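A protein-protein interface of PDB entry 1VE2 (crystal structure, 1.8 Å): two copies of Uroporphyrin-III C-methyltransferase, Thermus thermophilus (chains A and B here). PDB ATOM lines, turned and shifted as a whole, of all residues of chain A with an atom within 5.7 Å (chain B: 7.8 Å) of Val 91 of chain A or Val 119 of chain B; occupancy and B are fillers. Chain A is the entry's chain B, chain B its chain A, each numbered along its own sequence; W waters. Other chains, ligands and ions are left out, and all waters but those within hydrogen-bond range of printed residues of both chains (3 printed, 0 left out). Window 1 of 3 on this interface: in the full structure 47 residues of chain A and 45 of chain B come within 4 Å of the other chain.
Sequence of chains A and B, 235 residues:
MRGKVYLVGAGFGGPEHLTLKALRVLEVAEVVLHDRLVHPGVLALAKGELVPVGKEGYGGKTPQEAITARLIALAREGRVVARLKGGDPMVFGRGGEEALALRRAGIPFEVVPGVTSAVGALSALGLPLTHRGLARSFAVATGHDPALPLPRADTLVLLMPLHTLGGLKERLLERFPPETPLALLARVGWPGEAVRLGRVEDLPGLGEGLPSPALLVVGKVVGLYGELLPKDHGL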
ATOM      1  N   ASP A  88       8.703   0.788  14.728  1.00  0.00           N
ATOM      2  CA  ASP A  88       8.566  -0.663  14.664  1.00  0.00           C
ATOM      3  C   ASP A  88       9.512  -1.285  15.695  1.00  0.00           C
ATOM      4  O   ASP A  88      10.659  -0.854  15.831  1.00  0.00           O
ATOM      5  CB  ASP A  88       8.903  -1.168  13.256  1.00  0.00           C
ATOM      6  CG  ASP A  88       8.812  -2.675  13.143  1.00  0.00           C
ATOM      7  OD1 ASP A  88       9.796  -3.355  13.498  1.00  0.00           O
ATOM      8  OD2 ASP A  88       7.748  -3.178  12.715  1.00  0.00           O
ATOM      9  N   PRO A  89       9.042  -2.315  16.427  1.00  0.00           N
ATOM     10  CA  PRO A  89       9.773  -3.047  17.471  1.00  0.00           C
ATOM     11  C   PRO A  89      11.100  -3.681  17.074  1.00  0.00           C
ATOM     12  O   PRO A  89      11.985  -3.840  17.913  1.00  0.00           O
ATOM     13  CB  PRO A  89       8.780  -4.130  17.916  1.00  0.00           C
ATOM     14  CG  PRO A  89       7.467  -3.628  17.495  1.00  0.00           C
ATOM     15  CD  PRO A  89       7.736  -2.949  16.182  1.00  0.00           C
ATOM     16  N   MET A  90      11.235  -4.057  15.808  1.00  0.00           N
ATOM     17  CA  MET A  90      12.450  -4.715  15.342  1.00  0.00           C
ATOM     18  C   MET A  90      13.378  -3.840  14.520  1.00  0.00           C
ATOM     19  O   MET A  90      14.442  -4.290  14.109  1.00  0.00           O
ATOM     20  CB  MET A  90      12.086  -5.945  14.511  1.00  0.00           C
ATOM     21  CG  MET A  90      11.154  -6.906  15.215  1.00  0.00           C
ATOM     22  SD  MET A  90      11.897  -7.589  16.715  1.00  0.00           S
ATOM     23  CE  MET A  90      13.017  -8.750  15.979  1.00  0.00           C
ATOM     24  N   VAL A  91      12.986  -2.598  14.274  1.00  0.00           N
ATOM     25  CA  VAL A  91      13.816  -1.716  13.471  1.00  0.00           C
ATOM     26  C   VAL A  91      14.707  -0.791  14.289  1.00  0.00           C
ATOM     27  O   VAL A  91      14.227   0.046  15.049  1.00  0.00           O
ATOM     28  CB  VAL A  91      12.953  -0.865  12.506  1.00  0.00           C
ATOM     29  CG1 VAL A  91      13.851   0.040  11.653  1.00  0.00           C
ATOM     30  CG2 VAL A  91      12.134  -1.777  11.607  1.00  0.00           C
ATOM     31  N   PHE A  92      16.013  -0.973  14.123  1.00  0.00           N
ATOM     32  CA  PHE A  92      17.036  -0.166  14.782  1.00  0.00           C
ATOM     33  C   PHE A  92      16.923   0.078  16.271  1.00  0.00           C
ATOM     34  O   PHE A  92      17.024   1.211  16.745  1.00  0.00           O
ATOM     35  CB  PHE A  92      17.185   1.179  14.076  1.00  0.00           C
ATOM     36  CG  PHE A  92      17.964   1.095  12.805  1.00  0.00           C
ATOM     37  CD1 PHE A  92      17.330   1.207  11.576  1.00  0.00           C
ATOM     38  CD2 PHE A  92      19.334   0.857  12.837  1.00  0.00           C
ATOM     39  CE1 PHE A  92      18.046   1.080  10.399  1.00  0.00           C
ATOM     40  CE2 PHE A  92      20.062   0.726  11.664  1.00  0.00           C
ATOM     41  CZ  PHE A  92      19.416   0.839  10.440  1.00  0.00           C
ATOM     42  N   GLY A  93      16.720  -0.994  17.012  1.00  0.00           N
ATOM     43  CA  GLY A  93      16.656  -0.872  18.448  1.00  0.00           C
ATOM     44  C   GLY A  93      17.464  -2.055  18.912  1.00  0.00           C
ATOM     45  O   GLY A  93      18.579  -2.296  18.446  1.00  0.00           O
ATOM     46  N   THR A 116       7.166   2.507  10.742  1.00  0.00           N
ATOM     47  CA  THR A 116       8.474   3.089  11.067  1.00  0.00           C
ATOM     48  C   THR A 116       8.533   4.589  10.779  1.00  0.00           C
ATOM     49  O   THR A 116       7.713   5.119  10.042  1.00  0.00           O
ATOM     50  CB  THR A 116       9.577   2.448  10.219  1.00  0.00           C
ATOM     51  OG1 THR A 116       9.428   2.887   8.861  1.00  0.00           O
ATOM     52  CG2 THR A 116       9.464   0.944  10.245  1.00  0.00           C
ATOM     53  N   VAL A 140      18.533   2.237   4.853  1.00  0.00           N
ATOM     54  CA  VAL A 140      18.311   2.914   6.132  1.00  0.00           C
ATOM     55  C   VAL A 140      19.456   2.558   7.075  1.00  0.00           C
ATOM     56  O   VAL A 140      19.901   1.406   7.125  1.00  0.00           O
ATOM     57  CB  VAL A 140      16.985   2.452   6.788  1.00  0.00           C
ATOM     58  CG1 VAL A 140      16.717   3.255   8.065  1.00  0.00           C
ATOM     59  CG2 VAL A 140      15.829   2.608   5.803  1.00  0.00           C
ATOM     60  N   LEU A 159      18.674   7.930  10.548  1.00  0.00           N
ATOM     61  CA  LEU A 159      18.043   8.295  11.813  1.00  0.00           C
ATOM     62  C   LEU A 159      19.262   8.814  12.582  1.00  0.00           C
ATOM     63  O   LEU A 159      20.184   8.053  12.860  1.00  0.00           O
ATOM     64  CB  LEU A 159      17.482   7.032  12.483  1.00  0.00           C
ATOM     65  CG  LEU A 159      16.721   6.128  11.497  1.00  0.00           C
ATOM     66  CD1 LEU A 159      16.419   4.757  12.115  1.00  0.00           C
ATOM     67  CD2 LEU A 159      15.444   6.838  11.070  1.00  0.00           C
ATOM     68  N   PHE B  12       0.980  -5.530   5.005  1.00  0.00           N
ATOM     69  CA  PHE B  12       1.465  -6.718   4.297  1.00  0.00           C
ATOM     70  C   PHE B  12       0.537  -7.936   4.351  1.00  0.00           C
ATOM     71  O   PHE B  12       0.693  -8.876   3.562  1.00  0.00           O
ATOM     72  CB  PHE B  12       2.831  -7.114   4.870  1.00  0.00           C
ATOM     73  CG  PHE B  12       2.756  -7.685   6.258  1.00  0.00           C
ATOM     74  CD1 PHE B  12       2.485  -9.036   6.459  1.00  0.00           C
ATOM     75  CD2 PHE B  12       2.875  -6.860   7.369  1.00  0.00           C
ATOM     76  CE1 PHE B  12       2.329  -9.552   7.744  1.00  0.00           C
ATOM     77  CE2 PHE B  12       2.720  -7.371   8.652  1.00  0.00           C
ATOM     78  CZ  PHE B  12       2.444  -8.720   8.840  1.00  0.00           C
ATOM     79  N   VAL B 115       2.004  -0.742   7.218  1.00  0.00           N
ATOM     80  CA  VAL B 115       3.152  -1.573   7.581  1.00  0.00           C
ATOM     81  C   VAL B 115       3.643  -2.160   6.249  1.00  0.00           C
ATOM     82  O   VAL B 115       2.878  -2.806   5.535  1.00  0.00           O
ATOM     83  CB  VAL B 115       2.712  -2.706   8.551  1.00  0.00           C
ATOM     84  CG1 VAL B 115       3.827  -3.703   8.738  1.00  0.00           C
ATOM     85  CG2 VAL B 115       2.328  -2.094   9.914  1.00  0.00           C
ATOM     86  N   THR B 116       4.910  -1.931   5.916  1.00  0.00           N
ATOM     87  CA  THR B 116       5.459  -2.383   4.635  1.00  0.00           C
ATOM     88  C   THR B 116       5.515  -3.877   4.379  1.00  0.00           C
ATOM     89  O   THR B 116       5.609  -4.689   5.304  1.00  0.00           O
ATOM     90  CB  THR B 116       6.870  -1.817   4.401  1.00  0.00           C
ATOM     91  OG1 THR B 116       7.760  -2.318   5.411  1.00  0.00           O
ATOM     92  CG2 THR B 116       6.837  -0.301   4.444  1.00  0.00           C
ATOM     93  N   SER B 117       5.464  -4.204   3.088  1.00  0.00           N
ATOM     94  CA  SER B 117       5.492  -5.572   2.574  1.00  0.00           C
ATOM     95  C   SER B 117       6.797  -6.271   2.886  1.00  0.00           C
ATOM     96  O   SER B 117       6.842  -7.497   2.946  1.00  0.00           O
ATOM     97  CB  SER B 117       5.297  -5.569   1.051  1.00  0.00           C
ATOM     98  OG  SER B 117       4.052  -5.000   0.675  1.00  0.00           O
ATOM     99  N   ALA B 118       7.860  -5.488   3.059  1.00  0.00           N
ATOM    100  CA  ALA B 118       9.171  -6.037   3.361  1.00  0.00           C
ATOM    101  C   ALA B 118       9.390  -6.006   4.866  1.00  0.00           C
ATOM    102  O   ALA B 118       9.050  -6.957   5.568  1.00  0.00           O
ATOM    103  CB  ALA B 118      10.259  -5.230   2.647  1.00  0.00           C
ATOM    104  N   VAL B 119       9.933  -4.892   5.352  1.00  0.00           N
ATOM    105  CA  VAL B 119      10.217  -4.693   6.768  1.00  0.00           C
ATOM    106  C   VAL B 119       9.094  -5.092   7.725  1.00  0.00           C
ATOM    107  O   VAL B 119       9.338  -5.712   8.760  1.00  0.00           O
ATOM    108  CB  VAL B 119      10.596  -3.214   7.033  1.00  0.00           C
ATOM    109  CG1 VAL B 119      10.805  -2.978   8.517  1.00  0.00           C
ATOM    110  CG2 VAL B 119      11.863  -2.857   6.253  1.00  0.00           C
ATOM    111  N   GLY B 120       7.866  -4.724   7.387  1.00  0.00           N
ATOM    112  CA  GLY B 120       6.743  -5.052   8.243  1.00  0.00           C
ATOM    113  C   GLY B 120       6.521  -6.544   8.391  1.00  0.00           C
ATOM    114  O   GLY B 120       6.271  -7.030   9.494  1.00  0.00           O
ATOM    115  N   ALA B 121       6.606  -7.278   7.283  1.00  0.00           N
ATOM    116  CA  ALA B 121       6.405  -8.723   7.317  1.00  0.00           C
ATOM    117  C   ALA B 121       7.476  -9.395   8.163  1.00  0.00           C
ATOM    118  O   ALA B 121       7.182 -10.263   8.985  1.00  0.00           O
ATOM    119  CB  ALA B 121       6.423  -9.297   5.899  1.00  0.00           C
ATOM    120  N   LEU B 122       8.728  -8.997   7.956  1.00  0.00           N
ATOM    121  CA  LEU B 122       9.831  -9.571   8.720  1.00  0.00           C
ATOM    122  C   LEU B 122       9.649  -9.318  10.220  1.00  0.00           C
ATOM    123  O   LEU B 122       9.863 -10.212  11.035  1.00  0.00           O
ATOM    124  CB  LEU B 122      11.156  -8.983   8.228  1.00  0.00           C
ATOM    125  CG  LEU B 122      11.450  -9.265   6.752  1.00  0.00           C
ATOM    126  CD1 LEU B 122      12.674  -8.496   6.310  1.00  0.00           C
ATOM    127  CD2 LEU B 122      11.671 -10.759   6.551  1.00  0.00           C
ATOM    128  N   SER B 123       9.253  -8.105  10.593  1.00  0.00           N
ATOM    129  CA  SER B 123       9.043  -7.809  12.006  1.00  0.00           C
ATOM    130  C   SER B 123       7.903  -8.665  12.556  1.00  0.00           C
ATOM    131  O   SER B 123       7.966  -9.139  13.688  1.00  0.00           O
ATOM    132  CB  SER B 123       8.718  -6.326  12.217  1.00  0.00           C
ATOM    133  OG  SER B 123       9.837  -5.507  11.912  1.00  0.00           O
ATOM    134  N   ALA B 124       6.856  -8.867  11.759  1.00  0.00           N
ATOM    135  CA  ALA B 124       5.731  -9.675  12.222  1.00  0.00           C
ATOM    136  C   ALA B 124       6.196 -11.081  12.593  1.00  0.00           C
ATOM    137  O   ALA B 124       5.621 -11.722  13.476  1.00  0.00           O
ATOM    138  CB  ALA B 124       4.643  -9.743  11.151  1.00  0.00           C
ATOM    139  N   LEU B 125       7.236 -11.559  11.915  1.00  0.00           N
ATOM    140  CA  LEU B 125       7.779 -12.881  12.196  1.00  0.00           C
ATOM    141  C   LEU B 125       8.863 -12.802  13.262  1.00  0.00           C
ATOM    142  O   LEU B 125       9.509 -13.804  13.574  1.00  0.00           O
ATOM    143  CB  LEU B 125       8.346 -13.516  10.926  1.00  0.00           C
ATOM    144  CG  LEU B 125       7.300 -13.921   9.882  1.00  0.00           C
ATOM    145  CD1 LEU B 125       7.981 -14.464   8.635  1.00  0.00           C
ATOM    146  CD2 LEU B 125       6.372 -14.961  10.479  1.00  0.00           C
ATOM    147  N   GLY B 126       9.044 -11.608  13.826  1.00  0.00           N
ATOM    148  CA  GLY B 126      10.044 -11.408  14.860  1.00  0.00           C
ATOM    149  C   GLY B 126      11.464 -11.525  14.344  1.00  0.00           C
ATOM    150  O   GLY B 126      12.365 -11.956  15.067  1.00  0.00           O
ATOM    151  N   LEU B 127      11.669 -11.135  13.091  1.00  0.00           N
ATOM    152  CA  LEU B 127      12.989 -11.214  12.482  1.00  0.00           C
ATOM    153  C   LEU B 127      13.598  -9.822  12.284  1.00  0.00           C
ATOM    154  O   LEU B 127      12.994  -8.959  11.652  1.00  0.00           O
ATOM    155  CB  LEU B 127      12.878 -11.930  11.139  1.00  0.00           C
ATOM    156  CG  LEU B 127      12.174 -13.289  11.204  1.00  0.00           C
ATOM    157  CD1 LEU B 127      12.041 -13.835   9.793  1.00  0.00           C
ATOM    158  CD2 LEU B 127      12.952 -14.253  12.090  1.00  0.00           C
ATOM    159  N   PRO B 128      14.810  -9.596  12.819  1.00  0.00           N
ATOM    160  CA  PRO B 128      15.507  -8.310  12.706  1.00  0.00           C
ATOM    161  C   PRO B 128      16.308  -8.165  11.410  1.00  0.00           C
ATOM    162  O   PRO B 128      16.741  -9.160  10.825  1.00  0.00           O
ATOM    163  CB  PRO B 128      16.406  -8.314  13.935  1.00  0.00           C
ATOM    164  CG  PRO B 128      16.849  -9.757  13.985  1.00  0.00           C
ATOM    165  CD  PRO B 128      15.551 -10.519  13.704  1.00  0.00           C
ATOM    166  N   LEU B 129      16.490  -6.921  10.966  1.00  0.00           N
ATOM    167  CA  LEU B 129      17.250  -6.615   9.760  1.00  0.00           C
ATOM    168  C   LEU B 129      18.629  -6.119  10.156  1.00  0.00           C
ATOM    169  O   LEU B 129      19.532  -6.037   9.335  1.00  0.00           O
ATOM    170  CB  LEU B 129      16.539  -5.542   8.926  1.00  0.00           C
ATOM    171  CG  LEU B 129      15.265  -6.035   8.236  1.00  0.00           C
ATOM    172  CD1 LEU B 129      14.578  -4.878   7.514  1.00  0.00           C
ATOM    173  CD2 LEU B 129      15.627  -7.150   7.260  1.00  0.00           C
ATOM    174  N   THR B 130      18.774  -5.768  11.429  1.00  0.00           N
ATOM    175  CA  THR B 130      20.048  -5.305  11.958  1.00  0.00           C
ATOM    176  C   THR B 130      20.240  -5.960  13.316  1.00  0.00           C
ATOM    177  O   THR B 130      19.265  -6.310  13.976  1.00  0.00           O
ATOM    178  CB  THR B 130      20.071  -3.776  12.132  1.00  0.00           C
ATOM    179  OG1 THR B 130      18.973  -3.374  12.961  1.00  0.00           O
ATOM    180  CG2 THR B 130      19.972  -3.084  10.770  1.00  0.00           C
ATOM    181  N   PHE B 138      20.384  -1.691   6.324  1.00  0.00           N
ATOM    182  CA  PHE B 138      19.676  -2.558   5.399  1.00  0.00           C
ATOM    183  C   PHE B 138      19.219  -1.773   4.173  1.00  0.00           C
ATOM    184  O   PHE B 138      19.072  -0.554   4.218  1.00  0.00           O
ATOM    185  CB  PHE B 138      18.499  -3.274   6.091  1.00  0.00           C
ATOM    186  CG  PHE B 138      17.348  -2.382   6.456  1.00  0.00           C
ATOM    187  CD1 PHE B 138      16.384  -2.045   5.509  1.00  0.00           C
ATOM    188  CD2 PHE B 138      17.212  -1.894   7.759  1.00  0.00           C
ATOM    189  CE1 PHE B 138      15.294  -1.232   5.849  1.00  0.00           C
ATOM    190  CE2 PHE B 138      16.131  -1.082   8.109  1.00  0.00           C
ATOM    191  CZ  PHE B 138      15.168  -0.749   7.154  1.00  0.00           C
ATOM    192  N   ALA B 139      19.060  -2.467   3.052  1.00  0.00           N
ATOM    193  CA  ALA B 139      18.606  -1.808   1.841  1.00  0.00           C
ATOM    194  C   ALA B 139      17.475  -2.639   1.274  1.00  0.00           C
ATOM    195  O   ALA B 139      17.410  -3.853   1.496  1.00  0.00           O
ATOM    196  CB  ALA B 139      19.739  -1.699   0.824  1.00  0.00           C
ATOM    197  N   VAL B 140      16.581  -1.984   0.553  1.00  0.00           N
ATOM    198  CA  VAL B 140      15.452  -2.674  -0.046  1.00  0.00           C
ATOM    199  C   VAL B 140      15.417  -2.360  -1.538  1.00  0.00           C
ATOM    200  O   VAL B 140      15.589  -1.211  -1.953  1.00  0.00           O
ATOM    201  CB  VAL B 140      14.115  -2.222   0.579  1.00  0.00           C
ATOM    202  CG1 VAL B 140      12.958  -3.031  -0.025  1.00  0.00           C
ATOM    203  CG2 VAL B 140      14.150  -2.401   2.101  1.00  0.00           C
ATOM    204  N   VAL B 157      17.273  -6.671   1.300  1.00  0.00           N
ATOM    205  CA  VAL B 157      15.921  -7.205   1.184  1.00  0.00           C
ATOM    206  C   VAL B 157      15.468  -6.995  -0.258  1.00  0.00           C
ATOM    207  O   VAL B 157      15.544  -5.885  -0.790  1.00  0.00           O
ATOM    208  CB  VAL B 157      14.927  -6.478   2.123  1.00  0.00           C
ATOM    209  CG1 VAL B 157      13.543  -7.109   2.012  1.00  0.00           C
ATOM    210  CG2 VAL B 157      15.426  -6.540   3.556  1.00  0.00           C
ATOM    211  N   LEU B 159      12.280  -7.529  -2.967  1.00  0.00           N
ATOM    212  CA  LEU B 159      10.871  -7.824  -3.141  1.00  0.00           C
ATOM    213  C   LEU B 159      10.741  -8.552  -4.474  1.00  0.00           C
ATOM    214  O   LEU B 159      11.370  -8.166  -5.460  1.00  0.00           O
ATOM    215  CB  LEU B 159      10.056  -6.527  -3.159  1.00  0.00           C
ATOM    216  CG  LEU B 159      10.295  -5.585  -1.964  1.00  0.00           C
ATOM    217  CD1 LEU B 159       9.569  -4.266  -2.166  1.00  0.00           C
ATOM    218  CD2 LEU B 159       9.826  -6.250  -0.691  1.00  0.00           C
ATOM    219  N   LEU B 215       9.533 -12.668  -0.489  1.00  0.00           N
ATOM    220  CA  LEU B 215      10.581 -11.742  -0.082  1.00  0.00           C
ATOM    221  C   LEU B 215      11.877 -12.515   0.063  1.00  0.00           C
ATOM    222  O   LEU B 215      11.867 -13.710   0.355  1.00  0.00           O
ATOM    223  CB  LEU B 215      10.274 -11.125   1.283  1.00  0.00           C
ATOM    224  CG  LEU B 215       9.048 -10.258   1.540  1.00  0.00           C
ATOM    225  CD1 LEU B 215       9.002  -9.887   3.021  1.00  0.00           C
ATOM    226  CD2 LEU B 215       9.109  -9.012   0.676  1.00  0.00           C
ATOM    227  N   VAL B 217      15.783 -12.108   1.933  1.00  0.00           N
ATOM    228  CA  VAL B 217      16.613 -11.356   2.867  1.00  0.00           C
ATOM    229  C   VAL B 217      17.963 -12.068   2.941  1.00  0.00           C
ATOM    230  O   VAL B 217      18.023 -13.267   3.225  1.00  0.00           O
ATOM    231  CB  VAL B 217      15.997 -11.306   4.284  1.00  0.00           C
ATOM    232  CG1 VAL B 217      16.825 -10.377   5.171  1.00  0.00           C
ATOM    233  CG2 VAL B 217      14.551 -10.844   4.214  1.00  0.00           C
HETATM  234  O   HOH W   1      16.695  -2.511  11.998  1.00  0.00           O
HETATM  235  O   HOH W   2      19.104  -3.359  16.135  1.00  0.00           O
HETATM  236  O   HOH W   3      14.634  -4.875  11.564  1.00  0.00           O
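Water W2 lies within hydrogen-bond range of the backbone carbonyl oxygen (O) of Gly 93 of chain A (2.6 Å) and the side-chain hydroxyl (OG1) of Thr 130 of chain B (3.2 Å).
Water W3 bridges the backbone carbonyl oxygen of Met 90 of chain A and the backbone NH of Leu 129 of chain B.
Water W1 bridges OG1 of Thr 130 of chain B and N of Phe 92 of chain A.
3 positions are printed for both chains.
Of the 9 pairs that touch across the chains among the printed residues, none has its exchanged pair printed and touching as well.
The backbone NH of Leu 127 of chain B is in hydrogen-bond range of the backbone carbonyl oxygen of Leu 122 of chain B, 2.9 Å away.
The side-chain carboxylate (OD1) of Asp 88 of chain A lies within hydrogen-bond range of the backbone NH (N) of Met 90 of chain A, 2.8 Å away.
The side-chain hydroxyl (OG1) of Thr 116 of chain B lies within hydrogen-bond range of the backbone NH (N) of Val 119 of chain B (3.4 Å).
OD1 of Asp 88 of chain A lies within hydrogen-bond range of N of Val 91 of chain A (3.4 Å).
The backbone carbonyl oxygen of Val 119 of chain B lies within hydrogen-bond range of the side-chain hydroxyl of Ser 123 of chain B (3.2 Å).
Among the printed residues, pairs that only touch across the chains: Met 90 of chain A with Gly 126 of chain B, Met 90 of chain A with Ser 123 of chain B, Val 91 of chain A with Val 119 of chain B, Phe 92 of chain A with Phe 138 of chain B, Met 90 of chain A with Pro 128 of chain B, Met 90 of chain A with Leu 127 of chain B and Phe 92 of chain A with Thr 130 of chain B.
Of the 24 printed residues of chain B, 7 touch a printed residue of chain A.
Hydrophobic or aromatic side chains of chain B within 4 Å of the printed part of chain A: Val 119, Pro 128 and Phe 138.
Along chain B the printed residues that touch a printed residue of chain A span positions 119 to 138.
Among the printed residues, 9 pairs touch across the chains.
Among the printed residues, no Asp or Glu carboxylate lies within 4 Å of a Lys or Arg side-chain nitrogen of the other chain.
Of chain A, only Val 91 (3.6 Å) comes within 4 Å of Val 119 of chain B.
Printed residues of chain A within 4 Å of Ser 123 of chain B: Asp 88 (2.7 Å) and Met 90 (3.5 Å).
Of the printed residues of chain A, Leu 127 of chain B touches Met 90.
Of the printed residues of chain A, Thr 130 of chain B touches Phe 92.
The nearest residue of chain B that does not touch Val 91 of chain A is Phe 138 of chain B (4.4 Å).
The nearest printed residue of chain B that does not touch Asp 88 of chain A is Gly 120 of chain B (5.0 Å).
The side-chain carboxylate (OD1) of Asp 88 of chain A sits at hydrogen-bond distance from the side-chain hydroxyl (OG) of Ser 123 of chain B (2.7 Å).
O of Phe 138 of chain B sits at hydrogen-bond distance from N of Val 140 of chain A (2.9 Å).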
